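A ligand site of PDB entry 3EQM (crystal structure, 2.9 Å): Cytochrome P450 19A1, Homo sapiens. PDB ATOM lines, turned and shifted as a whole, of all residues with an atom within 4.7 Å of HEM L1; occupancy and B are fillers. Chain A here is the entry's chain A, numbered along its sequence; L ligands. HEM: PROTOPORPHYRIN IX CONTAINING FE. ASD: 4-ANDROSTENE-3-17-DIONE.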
ATOM      1  N   MET A 107      12.671 -11.201   8.943  1.00  0.00           N
ATOM      2  CA  MET A 107      13.685 -10.406   8.247  1.00  0.00           C
ATOM      3  C   MET A 107      14.273  -9.333   9.144  1.00  0.00           C
ATOM      4  O   MET A 107      15.381  -8.827   8.894  1.00  0.00           O
ATOM      5  CB  MET A 107      13.107  -9.797   6.967  1.00  0.00           C
ATOM      6  CG  MET A 107      12.343 -10.780   6.113  1.00  0.00           C
ATOM      7  SD  MET A 107      12.035 -10.287   4.408  1.00  0.00           S
ATOM      8  CE  MET A 107      11.906  -8.535   4.561  1.00  0.00           C
ATOM      9  N   ARG A 115      20.257 -18.868   5.240  1.00  0.00           N
ATOM     10  CA  ARG A 115      19.373 -19.573   4.301  1.00  0.00           C
ATOM     11  C   ARG A 115      19.578 -21.069   4.519  1.00  0.00           C
ATOM     12  O   ARG A 115      20.189 -21.481   5.512  1.00  0.00           O
ATOM     13  CB  ARG A 115      19.683 -19.190   2.834  1.00  0.00           C
ATOM     14  CG  ARG A 115      19.774 -17.701   2.585  1.00  0.00           C
ATOM     15  CD  ARG A 115      19.532 -17.321   1.129  1.00  0.00           C
ATOM     16  NE  ARG A 115      19.796 -15.906   0.913  1.00  0.00           N
ATOM     17  CZ  ARG A 115      18.950 -14.908   1.205  1.00  0.00           C
ATOM     18  NH1 ARG A 115      17.750 -15.166   1.706  1.00  0.00           N
ATOM     19  NH2 ARG A 115      19.296 -13.647   0.980  1.00  0.00           N
ATOM     20  N   ILE A 132      27.998 -14.859  -0.678  1.00  0.00           N
ATOM     21  CA  ILE A 132      27.038 -14.444   0.318  1.00  0.00           C
ATOM     22  C   ILE A 132      25.653 -15.044   0.085  1.00  0.00           C
ATOM     23  O   ILE A 132      25.008 -15.442   1.047  1.00  0.00           O
ATOM     24  CB  ILE A 132      26.942 -12.914   0.538  1.00  0.00           C
ATOM     25  CG1 ILE A 132      26.534 -12.160  -0.725  1.00  0.00           C
ATOM     26  CG2 ILE A 132      28.238 -12.361   1.132  1.00  0.00           C
ATOM     27  CD1 ILE A 132      25.948 -10.820  -0.364  1.00  0.00           C
ATOM     28  N   ILE A 133      25.209 -15.128  -1.171  1.00  0.00           N
ATOM     29  CA  ILE A 133      23.820 -15.477  -1.468  1.00  0.00           C
ATOM     30  C   ILE A 133      23.314 -16.676  -0.639  1.00  0.00           C
ATOM     31  O   ILE A 133      22.337 -16.565   0.086  1.00  0.00           O
ATOM     32  CB  ILE A 133      23.557 -15.686  -2.967  1.00  0.00           C
ATOM     33  CG1 ILE A 133      24.018 -14.466  -3.762  1.00  0.00           C
ATOM     34  CG2 ILE A 133      22.083 -15.906  -3.237  1.00  0.00           C
ATOM     35  CD1 ILE A 133      24.243 -14.749  -5.240  1.00  0.00           C
ATOM     36  N   TRP A 141      29.676 -15.264   6.513  1.00  0.00           N
ATOM     37  CA  TRP A 141      28.719 -14.395   5.848  1.00  0.00           C
ATOM     38  C   TRP A 141      28.844 -12.967   6.361  1.00  0.00           C
ATOM     39  O   TRP A 141      29.021 -12.036   5.570  1.00  0.00           O
ATOM     40  CB  TRP A 141      27.291 -14.908   6.039  1.00  0.00           C
ATOM     41  CG  TRP A 141      26.221 -13.921   5.636  1.00  0.00           C
ATOM     42  CD1 TRP A 141      25.802 -13.624   4.367  1.00  0.00           C
ATOM     43  CD2 TRP A 141      25.432 -13.115   6.513  1.00  0.00           C
ATOM     44  NE1 TRP A 141      24.794 -12.680   4.411  1.00  0.00           N
ATOM     45  CE2 TRP A 141      24.562 -12.349   5.714  1.00  0.00           C
ATOM     46  CE3 TRP A 141      25.396 -12.949   7.905  1.00  0.00           C
ATOM     47  CZ2 TRP A 141      23.636 -11.442   6.263  1.00  0.00           C
ATOM     48  CZ3 TRP A 141      24.480 -12.057   8.440  1.00  0.00           C
ATOM     49  CH2 TRP A 141      23.618 -11.306   7.627  1.00  0.00           C
ATOM     50  N   ARG A 145      29.627  -9.931   3.654  1.00  0.00           N
ATOM     51  CA  ARG A 145      28.572  -9.019   3.232  1.00  0.00           C
ATOM     52  C   ARG A 145      29.028  -7.543   3.096  1.00  0.00           C
ATOM     53  O   ARG A 145      28.682  -6.886   2.119  1.00  0.00           O
ATOM     54  CB  ARG A 145      27.344  -9.162   4.135  1.00  0.00           C
ATOM     55  CG  ARG A 145      26.139  -8.429   3.610  1.00  0.00           C
ATOM     56  CD  ARG A 145      24.879  -8.936   4.223  1.00  0.00           C
ATOM     57  NE  ARG A 145      23.832  -7.908   4.228  1.00  0.00           N
ATOM     58  CZ  ARG A 145      22.789  -7.862   3.396  1.00  0.00           C
ATOM     59  NH1 ARG A 145      22.619  -8.795   2.459  1.00  0.00           N
ATOM     60  NH2 ARG A 145      21.913  -6.885   3.516  1.00  0.00           N
ATOM     61  N   PHE A 148      29.932  -6.356  -0.343  1.00  0.00           N
ATOM     62  CA  PHE A 148      28.844  -6.191  -1.278  1.00  0.00           C
ATOM     63  C   PHE A 148      28.097  -4.907  -0.988  1.00  0.00           C
ATOM     64  O   PHE A 148      27.765  -4.166  -1.915  1.00  0.00           O
ATOM     65  CB  PHE A 148      27.891  -7.387  -1.219  1.00  0.00           C
ATOM     66  CG  PHE A 148      28.396  -8.606  -1.936  1.00  0.00           C
ATOM     67  CD1 PHE A 148      29.225  -9.514  -1.281  1.00  0.00           C
ATOM     68  CD2 PHE A 148      28.034  -8.851  -3.246  1.00  0.00           C
ATOM     69  CE1 PHE A 148      29.687 -10.650  -1.935  1.00  0.00           C
ATOM     70  CE2 PHE A 148      28.493  -9.975  -3.921  1.00  0.00           C
ATOM     71  CZ  PHE A 148      29.322 -10.877  -3.258  1.00  0.00           C
ATOM     72  N   LEU A 152      27.666  -1.532  -3.659  1.00  0.00           N
ATOM     73  CA  LEU A 152      26.291  -1.373  -4.165  1.00  0.00           C
ATOM     74  C   LEU A 152      25.553  -0.124  -3.648  1.00  0.00           C
ATOM     75  O   LEU A 152      24.328  -0.001  -3.800  1.00  0.00           O
ATOM     76  CB  LEU A 152      25.469  -2.648  -3.858  1.00  0.00           C
ATOM     77  CG  LEU A 152      25.939  -3.959  -4.505  1.00  0.00           C
ATOM     78  CD1 LEU A 152      25.205  -5.125  -3.890  1.00  0.00           C
ATOM     79  CD2 LEU A 152      25.775  -3.925  -6.012  1.00  0.00           C
ATOM     80  N   PHE A 203      32.067  -3.316 -11.298  1.00  0.00           N
ATOM     81  CA  PHE A 203      32.622  -4.078 -10.165  1.00  0.00           C
ATOM     82  C   PHE A 203      33.951  -4.774 -10.420  1.00  0.00           C
ATOM     83  O   PHE A 203      34.662  -5.113  -9.481  1.00  0.00           O
ATOM     84  CB  PHE A 203      31.618  -5.101  -9.623  1.00  0.00           C
ATOM     85  CG  PHE A 203      30.250  -4.547  -9.387  1.00  0.00           C
ATOM     86  CD1 PHE A 203      30.047  -3.518  -8.474  1.00  0.00           C
ATOM     87  CD2 PHE A 203      29.142  -5.076 -10.060  1.00  0.00           C
ATOM     88  CE1 PHE A 203      28.776  -3.004  -8.244  1.00  0.00           C
ATOM     89  CE2 PHE A 203      27.867  -4.582  -9.840  1.00  0.00           C
ATOM     90  CZ  PHE A 203      27.682  -3.541  -8.937  1.00  0.00           C
ATOM     91  N   MET A 303      28.698 -11.531  -7.797  1.00  0.00           N
ATOM     92  CA  MET A 303      28.462 -10.143  -8.160  1.00  0.00           C
ATOM     93  C   MET A 303      28.150  -9.990  -9.658  1.00  0.00           C
ATOM     94  O   MET A 303      27.361  -9.131 -10.049  1.00  0.00           O
ATOM     95  CB  MET A 303      29.662  -9.292  -7.767  1.00  0.00           C
ATOM     96  CG  MET A 303      29.492  -7.784  -7.982  1.00  0.00           C
ATOM     97  SD  MET A 303      28.126  -7.076  -7.022  1.00  0.00           S
ATOM     98  CE  MET A 303      28.984  -6.426  -5.602  1.00  0.00           C
ATOM     99  N   ALA A 306      24.428 -11.743 -10.587  1.00  0.00           N
ATOM    100  CA  ALA A 306      23.254 -11.236  -9.875  1.00  0.00           C
ATOM    101  C   ALA A 306      22.262 -10.481 -10.767  1.00  0.00           C
ATOM    102  O   ALA A 306      21.092 -10.853 -10.844  1.00  0.00           O
ATOM    103  CB  ALA A 306      23.671 -10.378  -8.679  1.00  0.00           C
ATOM    104  N   ALA A 307      22.724  -9.434 -11.432  1.00  0.00           N
ATOM    105  CA  ALA A 307      21.844  -8.622 -12.266  1.00  0.00           C
ATOM    106  C   ALA A 307      21.347  -9.367 -13.523  1.00  0.00           C
ATOM    107  O   ALA A 307      20.141  -9.420 -13.754  1.00  0.00           O
ATOM    108  CB  ALA A 307      22.502  -7.294 -12.627  1.00  0.00           C
ATOM    109  N   THR A 310      18.470 -11.692 -12.271  1.00  0.00           N
ATOM    110  CA  THR A 310      17.206 -11.160 -11.780  1.00  0.00           C
ATOM    111  C   THR A 310      16.680  -9.931 -12.525  1.00  0.00           C
ATOM    112  O   THR A 310      15.480  -9.841 -12.777  1.00  0.00           O
ATOM    113  CB  THR A 310      17.283 -10.826 -10.288  1.00  0.00           C
ATOM    114  OG1 THR A 310      18.580 -10.259  -9.994  1.00  0.00           O
ATOM    115  CG2 THR A 310      17.096 -12.085  -9.475  1.00  0.00           C
ATOM    116  N   MET A 311      17.582  -8.995 -12.839  1.00  0.00           N
ATOM    117  CA  MET A 311      17.195  -7.713 -13.424  1.00  0.00           C
ATOM    118  C   MET A 311      16.624  -7.865 -14.817  1.00  0.00           C
ATOM    119  O   MET A 311      15.614  -7.250 -15.139  1.00  0.00           O
ATOM    120  CB  MET A 311      18.395  -6.779 -13.508  1.00  0.00           C
ATOM    121  CG  MET A 311      18.827  -6.247 -12.165  1.00  0.00           C
ATOM    122  SD  MET A 311      18.068  -4.661 -11.840  1.00  0.00           S
ATOM    123  CE  MET A 311      18.791  -3.695 -13.156  1.00  0.00           C
ATOM    124  N   SER A 314      13.236  -9.431 -14.708  1.00  0.00           N
ATOM    125  CA  SER A 314      12.385  -8.375 -14.146  1.00  0.00           C
ATOM    126  C   SER A 314      12.002  -7.332 -15.189  1.00  0.00           C
ATOM    127  O   SER A 314      10.833  -7.012 -15.364  1.00  0.00           O
ATOM    128  CB  SER A 314      13.076  -7.690 -12.967  1.00  0.00           C
ATOM    129  OG  SER A 314      12.901  -8.451 -11.789  1.00  0.00           O
ATOM    130  N   MET A 364       6.756  -5.495 -10.080  1.00  0.00           N
ATOM    131  CA  MET A 364       7.355  -6.448  -9.153  1.00  0.00           C
ATOM    132  C   MET A 364       6.336  -7.069  -8.214  1.00  0.00           C
ATOM    133  O   MET A 364       6.438  -8.259  -7.889  1.00  0.00           O
ATOM    134  CB  MET A 364       8.463  -5.785  -8.356  1.00  0.00           C
ATOM    135  CG  MET A 364       9.750  -5.623  -9.123  1.00  0.00           C
ATOM    136  SD  MET A 364      10.953  -4.677  -8.175  1.00  0.00           S
ATOM    137  CE  MET A 364      11.531  -5.921  -7.041  1.00  0.00           C
ATOM    138  N   VAL A 370      11.450 -12.786  -8.065  1.00  0.00           N
ATOM    139  CA  VAL A 370      11.882 -13.312  -6.787  1.00  0.00           C
ATOM    140  C   VAL A 370      10.690 -13.302  -5.836  1.00  0.00           C
ATOM    141  O   VAL A 370      10.532 -12.428  -4.994  1.00  0.00           O
ATOM    142  CB  VAL A 370      13.080 -12.518  -6.238  1.00  0.00           C
ATOM    143  CG1 VAL A 370      13.696 -13.235  -5.077  1.00  0.00           C
ATOM    144  CG2 VAL A 370      14.122 -12.292  -7.331  1.00  0.00           C
ATOM    145  N   VAL A 373      11.635 -16.205  -0.546  1.00  0.00           N
ATOM    146  CA  VAL A 373      12.894 -15.997   0.157  1.00  0.00           C
ATOM    147  C   VAL A 373      13.133 -17.180   1.080  1.00  0.00           C
ATOM    148  O   VAL A 373      12.240 -17.578   1.827  1.00  0.00           O
ATOM    149  CB  VAL A 373      12.888 -14.672   0.948  1.00  0.00           C
ATOM    150  CG1 VAL A 373      14.190 -14.466   1.692  1.00  0.00           C
ATOM    151  CG2 VAL A 373      12.636 -13.493   0.028  1.00  0.00           C
ATOM    152  N   ARG A 375      15.035 -18.882   4.251  1.00  0.00           N
ATOM    153  CA  ARG A 375      15.742 -18.602   5.511  1.00  0.00           C
ATOM    154  C   ARG A 375      15.850 -19.844   6.414  1.00  0.00           C
ATOM    155  O   ARG A 375      15.304 -20.907   6.111  1.00  0.00           O
ATOM    156  CB  ARG A 375      15.065 -17.456   6.269  1.00  0.00           C
ATOM    157  CG  ARG A 375      14.917 -16.126   5.512  1.00  0.00           C
ATOM    158  CD  ARG A 375      16.248 -15.516   5.134  1.00  0.00           C
ATOM    159  NE  ARG A 375      16.142 -14.089   4.818  1.00  0.00           N
ATOM    160  CZ  ARG A 375      16.303 -13.116   5.713  1.00  0.00           C
ATOM    161  NH1 ARG A 375      16.564 -13.408   6.977  1.00  0.00           N
ATOM    162  NH2 ARG A 375      16.206 -11.844   5.339  1.00  0.00           N
ATOM    163  N   ILE A 398       6.680 -14.372  -0.587  1.00  0.00           N
ATOM    164  CA  ILE A 398       6.348 -12.953  -0.686  1.00  0.00           C
ATOM    165  C   ILE A 398       5.424 -12.618  -1.861  1.00  0.00           C
ATOM    166  O   ILE A 398       4.687 -11.629  -1.812  1.00  0.00           O
ATOM    167  CB  ILE A 398       7.584 -12.031  -0.622  1.00  0.00           C
ATOM    168  CG1 ILE A 398       8.560 -12.330  -1.757  1.00  0.00           C
ATOM    169  CG2 ILE A 398       8.265 -12.165   0.750  1.00  0.00           C
ATOM    170  CD1 ILE A 398       9.616 -11.255  -2.000  1.00  0.00           C
ATOM    171  N   PRO A 429       9.545  -6.375  -1.869  1.00  0.00           N
ATOM    172  CA  PRO A 429      10.044  -6.918  -3.123  1.00  0.00           C
ATOM    173  C   PRO A 429      11.524  -7.325  -3.056  1.00  0.00           C
ATOM    174  O   PRO A 429      11.966  -8.173  -3.841  1.00  0.00           O
ATOM    175  CB  PRO A 429       9.862  -5.763  -4.099  1.00  0.00           C
ATOM    176  CG  PRO A 429       9.879  -4.540  -3.269  1.00  0.00           C
ATOM    177  CD  PRO A 429       9.261  -4.932  -1.960  1.00  0.00           C
ATOM    178  N   PHE A 430      12.267  -6.735  -2.130  1.00  0.00           N
ATOM    179  CA  PHE A 430      13.706  -6.936  -2.031  1.00  0.00           C
ATOM    180  C   PHE A 430      14.123  -7.590  -0.718  1.00  0.00           C
ATOM    181  O   PHE A 430      15.274  -7.983  -0.563  1.00  0.00           O
ATOM    182  CB  PHE A 430      14.435  -5.586  -2.121  1.00  0.00           C
ATOM    183  CG  PHE A 430      14.345  -4.934  -3.455  1.00  0.00           C
ATOM    184  CD1 PHE A 430      13.503  -3.845  -3.646  1.00  0.00           C
ATOM    185  CD2 PHE A 430      15.111  -5.380  -4.530  1.00  0.00           C
ATOM    186  CE1 PHE A 430      13.423  -3.202  -4.898  1.00  0.00           C
ATOM    187  CE2 PHE A 430      15.036  -4.754  -5.782  1.00  0.00           C
ATOM    188  CZ  PHE A 430      14.190  -3.666  -5.959  1.00  0.00           C
ATOM    189  N   GLY A 431      13.194  -7.671   0.228  1.00  0.00           N
ATOM    190  CA  GLY A 431      13.555  -7.966   1.607  1.00  0.00           C
ATOM    191  C   GLY A 431      14.177  -6.731   2.257  1.00  0.00           C
ATOM    192  O   GLY A 431      14.616  -5.808   1.573  1.00  0.00           O
ATOM    193  N   PHE A 432      14.203  -6.720   3.591  1.00  0.00           N
ATOM    194  CA  PHE A 432      14.827  -5.658   4.371  1.00  0.00           C
ATOM    195  C   PHE A 432      15.526  -6.328   5.561  1.00  0.00           C
ATOM    196  O   PHE A 432      15.301  -7.510   5.827  1.00  0.00           O
ATOM    197  CB  PHE A 432      13.760  -4.677   4.889  1.00  0.00           C
ATOM    198  CG  PHE A 432      13.064  -5.163   6.130  1.00  0.00           C
ATOM    199  CD1 PHE A 432      13.540  -4.792   7.395  1.00  0.00           C
ATOM    200  CD2 PHE A 432      11.980  -6.019   6.055  1.00  0.00           C
ATOM    201  CE1 PHE A 432      12.921  -5.263   8.562  1.00  0.00           C
ATOM    202  CE2 PHE A 432      11.361  -6.501   7.207  1.00  0.00           C
ATOM    203  CZ  PHE A 432      11.841  -6.123   8.466  1.00  0.00           C
ATOM    204  N   ARG A 435      19.838  -9.175   6.390  1.00  0.00           N
ATOM    205  CA  ARG A 435      20.104 -10.027   5.218  1.00  0.00           C
ATOM    206  C   ARG A 435      19.152  -9.751   4.038  1.00  0.00           C
ATOM    207  O   ARG A 435      18.835 -10.651   3.262  1.00  0.00           O
ATOM    208  CB  ARG A 435      20.088 -11.510   5.614  1.00  0.00           C
ATOM    209  CG  ARG A 435      20.547 -12.448   4.508  1.00  0.00           C
ATOM    210  CD  ARG A 435      21.177 -13.712   5.043  1.00  0.00           C
ATOM    211  NE  ARG A 435      21.937 -14.380   3.973  1.00  0.00           N
ATOM    212  CZ  ARG A 435      22.778 -15.402   4.163  1.00  0.00           C
ATOM    213  NH1 ARG A 435      22.989 -15.900   5.370  1.00  0.00           N
ATOM    214  NH2 ARG A 435      23.403 -15.928   3.123  1.00  0.00           N
ATOM    215  N   GLY A 436      18.691  -8.505   3.893  1.00  0.00           N
ATOM    216  CA  GLY A 436      17.826  -8.138   2.782  1.00  0.00           C
ATOM    217  C   GLY A 436      18.653  -7.974   1.522  1.00  0.00           C
ATOM    218  O   GLY A 436      19.893  -7.926   1.607  1.00  0.00           O
ATOM    219  N   CYS A 437      18.013  -7.889   0.362  1.00  0.00           N
ATOM    220  CA  CYS A 437      18.736  -7.785  -0.903  1.00  0.00           C
ATOM    221  C   CYS A 437      19.865  -6.773  -0.771  1.00  0.00           C
ATOM    222  O   CYS A 437      19.617  -5.608  -0.476  1.00  0.00           O
ATOM    223  CB  CYS A 437      17.813  -7.396  -2.057  1.00  0.00           C
ATOM    224  SG  CYS A 437      18.670  -6.992  -3.587  1.00  0.00           S
ATOM    225  N   ALA A 438      21.100  -7.226  -0.997  1.00  0.00           N
ATOM    226  CA  ALA A 438      22.255  -6.352  -0.924  1.00  0.00           C
ATOM    227  C   ALA A 438      22.181  -5.250  -1.972  1.00  0.00           C
ATOM    228  O   ALA A 438      22.716  -4.165  -1.774  1.00  0.00           O
ATOM    229  CB  ALA A 438      23.532  -7.157  -1.108  1.00  0.00           C
ATOM    230  N   GLY A 439      21.513  -5.530  -3.081  1.00  0.00           N
ATOM    231  CA  GLY A 439      21.454  -4.588  -4.171  1.00  0.00           C
ATOM    232  C   GLY A 439      20.150  -3.851  -4.274  1.00  0.00           C
ATOM    233  O   GLY A 439      19.831  -3.300  -5.320  1.00  0.00           O
ATOM    234  N   ALA A 443      19.433  -1.514  -7.491  1.00  0.00           N
ATOM    235  CA  ALA A 443      18.531  -2.189  -8.403  1.00  0.00           C
ATOM    236  C   ALA A 443      17.482  -1.225  -8.965  1.00  0.00           C
ATOM    237  O   ALA A 443      17.181  -1.253 -10.162  1.00  0.00           O
ATOM    238  CB  ALA A 443      17.864  -3.370  -7.727  1.00  0.00           C
ATOM    239  N   MET A 446      19.180   1.162 -11.438  1.00  0.00           N
ATOM    240  CA  MET A 446      19.458   0.493 -12.698  1.00  0.00           C
ATOM    241  C   MET A 446      18.201   0.298 -13.524  1.00  0.00           C
ATOM    242  O   MET A 446      18.193   0.561 -14.715  1.00  0.00           O
ATOM    243  CB  MET A 446      20.124  -0.836 -12.440  1.00  0.00           C
ATOM    244  CG  MET A 446      21.561  -0.716 -12.007  1.00  0.00           C
ATOM    245  SD  MET A 446      22.368  -2.313 -11.833  1.00  0.00           S
ATOM    246  CE  MET A 446      21.889  -2.701 -10.163  1.00  0.00           C
ATOM    247  N   MET A 447      17.137  -0.165 -12.867  1.00  0.00           N
ATOM    248  CA  MET A 447      15.880  -0.397 -13.565  1.00  0.00           C
ATOM    249  C   MET A 447      15.280   0.871 -14.128  1.00  0.00           C
ATOM    250  O   MET A 447      14.680   0.847 -15.193  1.00  0.00           O
ATOM    251  CB  MET A 447      14.875  -1.117 -12.676  1.00  0.00           C
ATOM    252  CG  MET A 447      15.113  -2.606 -12.676  1.00  0.00           C
ATOM    253  SD  MET A 447      13.896  -3.534 -11.755  1.00  0.00           S
ATOM    254  CE  MET A 447      14.273  -3.054 -10.072  1.00  0.00           C
HETATM  255  CHA HEM L   1      19.188 -11.202  -2.127  1.00  0.00           C
HETATM  256  CHB HEM L   1      15.501  -9.481  -4.721  1.00  0.00           C
HETATM  257  CHC HEM L   1      18.636  -7.376  -7.686  1.00  0.00           C
HETATM  258  CHD HEM L   1      22.342  -8.883  -5.028  1.00  0.00           C
HETATM  259  C1A HEM L   1      17.917 -10.879  -2.543  1.00  0.00           C
HETATM  260  C2A HEM L   1      16.674 -11.203  -1.854  1.00  0.00           C
HETATM  261  C3A HEM L   1      15.653 -10.716  -2.568  1.00  0.00           C
HETATM  262  C4A HEM L   1      16.229 -10.072  -3.729  1.00  0.00           C
HETATM  263  CMA HEM L   1      14.150 -10.816  -2.251  1.00  0.00           C
HETATM  264  CAA HEM L   1      16.538 -11.958  -0.518  1.00  0.00           C
HETATM  265  CBA HEM L   1      16.600 -10.942   0.620  1.00  0.00           C
HETATM  266  CGA HEM L   1      16.281 -11.608   1.937  1.00  0.00           C
HETATM  267  O1A HEM L   1      16.752 -12.754   2.168  1.00  0.00           O
HETATM  268  O2A HEM L   1      15.566 -10.978   2.772  1.00  0.00           O
HETATM  269  C1B HEM L   1      16.031  -8.852  -5.808  1.00  0.00           C
HETATM  270  C2B HEM L   1      15.301  -8.389  -6.954  1.00  0.00           C
HETATM  271  C3B HEM L   1      16.185  -7.804  -7.779  1.00  0.00           C
HETATM  272  C4B HEM L   1      17.480  -7.882  -7.147  1.00  0.00           C
HETATM  273  CMB HEM L   1      13.776  -8.554  -7.165  1.00  0.00           C
HETATM  274  CAB HEM L   1      15.945  -7.150  -9.155  1.00  0.00           C
HETATM  275  CBB HEM L   1      14.793  -6.535  -9.427  1.00  0.00           C
HETATM  276  C1C HEM L   1      19.904  -7.542  -7.188  1.00  0.00           C
HETATM  277  C2C HEM L   1      21.111  -6.944  -7.733  1.00  0.00           C
HETATM  278  C3C HEM L   1      22.142  -7.372  -6.989  1.00  0.00           C
HETATM  279  C4C HEM L   1      21.604  -8.247  -5.966  1.00  0.00           C
HETATM  280  CMC HEM L   1      21.149  -5.998  -8.951  1.00  0.00           C
HETATM  281  CAC HEM L   1      23.645  -7.029  -7.126  1.00  0.00           C
HETATM  282  CBC HEM L   1      24.232  -6.857  -8.318  1.00  0.00           C
HETATM  283  C1D HEM L   1      21.846  -9.682  -4.037  1.00  0.00           C
HETATM  284  C2D HEM L   1      22.676 -10.420  -3.121  1.00  0.00           C
HETATM  285  C3D HEM L   1      21.710 -11.157  -2.194  1.00  0.00           C
HETATM  286  C4D HEM L   1      20.382 -10.780  -2.664  1.00  0.00           C
HETATM  287  CMD HEM L   1      24.214 -10.439  -3.110  1.00  0.00           C
HETATM  288  CAD HEM L   1      22.099 -12.088  -1.035  1.00  0.00           C
HETATM  289  CBD HEM L   1      21.986 -11.275   0.256  1.00  0.00           C
HETATM  290  CGD HEM L   1      22.417 -12.064   1.470  1.00  0.00           C
HETATM  291  O1D HEM L   1      23.171 -11.500   2.315  1.00  0.00           O
HETATM  292  O2D HEM L   1      21.987 -13.243   1.607  1.00  0.00           O
HETATM  293  NA  HEM L   1      17.604 -10.178  -3.690  1.00  0.00           N
HETATM  294  NB  HEM L   1      17.356  -8.534  -5.952  1.00  0.00           N
HETATM  295  NC  HEM L   1      20.229  -8.329  -6.113  1.00  0.00           N
HETATM  296  ND  HEM L   1      20.509  -9.920  -3.741  1.00  0.00           N
HETATM  297 FE   HEM L   1      18.910  -9.058  -4.780  1.00  0.00          FE
HETATM  298  C1  ASD L   2      20.376 -13.638  -5.906  1.00  0.00           C
HETATM  299  C10 ASD L   2      18.903 -14.023  -6.126  1.00  0.00           C
HETATM  300  C11 ASD L   2      18.605 -14.471  -3.631  1.00  0.00           C
HETATM  301  C12 ASD L   2      18.144 -15.418  -2.529  1.00  0.00           C
HETATM  302  C13 ASD L   2      16.755 -15.919  -2.848  1.00  0.00           C
HETATM  303  C14 ASD L   2      16.791 -16.636  -4.186  1.00  0.00           C
HETATM  304  C15 ASD L   2      15.525 -17.495  -4.222  1.00  0.00           C
HETATM  305  C16 ASD L   2      15.413 -18.034  -2.798  1.00  0.00           C
HETATM  306  C17 ASD L   2      16.224 -17.042  -1.989  1.00  0.00           C
HETATM  307  C18 ASD L   2      15.713 -14.792  -2.780  1.00  0.00           C
HETATM  308  C19 ASD L   2      18.028 -12.770  -6.014  1.00  0.00           C
HETATM  309  C2  ASD L   2      21.040 -13.029  -7.128  1.00  0.00           C
HETATM  310  C3  ASD L   2      20.842 -13.982  -8.289  1.00  0.00           C
HETATM  311  C4  ASD L   2      19.622 -14.548  -8.496  1.00  0.00           C
HETATM  312  C5  ASD L   2      18.696 -14.653  -7.506  1.00  0.00           C
HETATM  313  C6  ASD L   2      17.428 -15.419  -7.813  1.00  0.00           C
HETATM  314  C7  ASD L   2      17.151 -16.412  -6.687  1.00  0.00           C
HETATM  315  C8  ASD L   2      17.130 -15.708  -5.339  1.00  0.00           C
HETATM  316  C9  ASD L   2      18.491 -15.044  -5.055  1.00  0.00           C
HETATM  317  O1  ASD L   2      21.790 -14.238  -9.029  1.00  0.00           O
HETATM  318  O2  ASD L   2      16.425 -17.127  -0.794  1.00  0.00           O
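The side-chain sulfur of Cys 437 binds an iron atom (FE) of HEM L1 (2.4 Å).
An oxygen (O2D) of HEM L1 is in salt-bridge range of the guanidinium group (NE) of Arg 435.
O1A of HEM L1 lies within salt-bridge range of NH1 of Arg 115 (2.7 Å).
An oxygen (O1D) of HEM L1 lies within salt-bridge range of the guanidinium group (NH1) of Arg 145 (2.8 Å).
The guanidinium group (NH2) of Arg 375 lies within salt-bridge range of an oxygen (O2A) of HEM L1 (2.8 Å).
O1D of HEM L1 lies within hydrogen-bond range of NE1 of Trp 141 (2.9 Å).
The guanidinium group (NH1) of Arg 115 lies within hydrogen-bond range of an oxygen (O2) of ASD L2.
The backbone carbonyl oxygen of Phe 430 sits at hydrogen-bond distance from the backbone NH of Cys 437, 2.9 Å away.
The side-chain sulfur of Cys 437 sits close to the backbone NH of Gly 439 (3.2 Å).
The backbone carbonyl oxygen (O) of Ile 132 is in hydrogen-bond range of the guanidinium group (NH2) of Arg 435 (2.7 Å).
The guanidinium group (NH2) of Arg 435 is in hydrogen-bond range of the backbone carbonyl oxygen (O) of Ile 133 (3.3 Å).
The guanidinium group (NE) of Arg 115 lies within hydrogen-bond range of the backbone carbonyl oxygen (O) of Ile 133, 2.8 Å away.
The guanidinium group of Arg 145 sits at hydrogen-bond distance from the backbone carbonyl oxygen of Gly 436, 3.0 Å away.
The side-chain hydroxyl of Ser 314 lies within hydrogen-bond range of the backbone carbonyl oxygen of Thr 310 (3.1 Å).
O of Ala 306 is in hydrogen-bond range of OG1 of Thr 310 (2.7 Å).
Residues that only touch HEM L1: Met 107 (3.95 Å), Ile 132 (3.3 Å), Ile 133 (3.7 Å), Leu 152 (3.9 Å), Ala 306 (3.6 Å), Thr 310 (3.7 Å), Met 311 (3.97 Å), Ser 314 (3.6 Å), Met 364 (3.5 Å), Val 370 (3.7 Å), Val 373 (3.1 Å), Pro 429 (3.8 Å), Phe 430 (3.4 Å), Gly 431 (3.8 Å), Gly 436 (3.6 Å), Ala 438 (3.9 Å), Gly 439 (3.96 Å), Met 446 (3.6 Å) and Met 447 (3.6 Å).
Hydrophobic or aromatic side chains within 4 Å of HEM L1: Met 107, Ile 132, Trp 141, Leu 152, Ala 306, Met 311, Met 364, Val 370, Val 373, Phe 430, Ala 438, Met 446 and Met 447.
Of the 32 residues printed, 25 come within 4 Å of HEM L1.
The nearest printed residue that does not touch HEM L1 is Ala 443 (4.1 Å).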
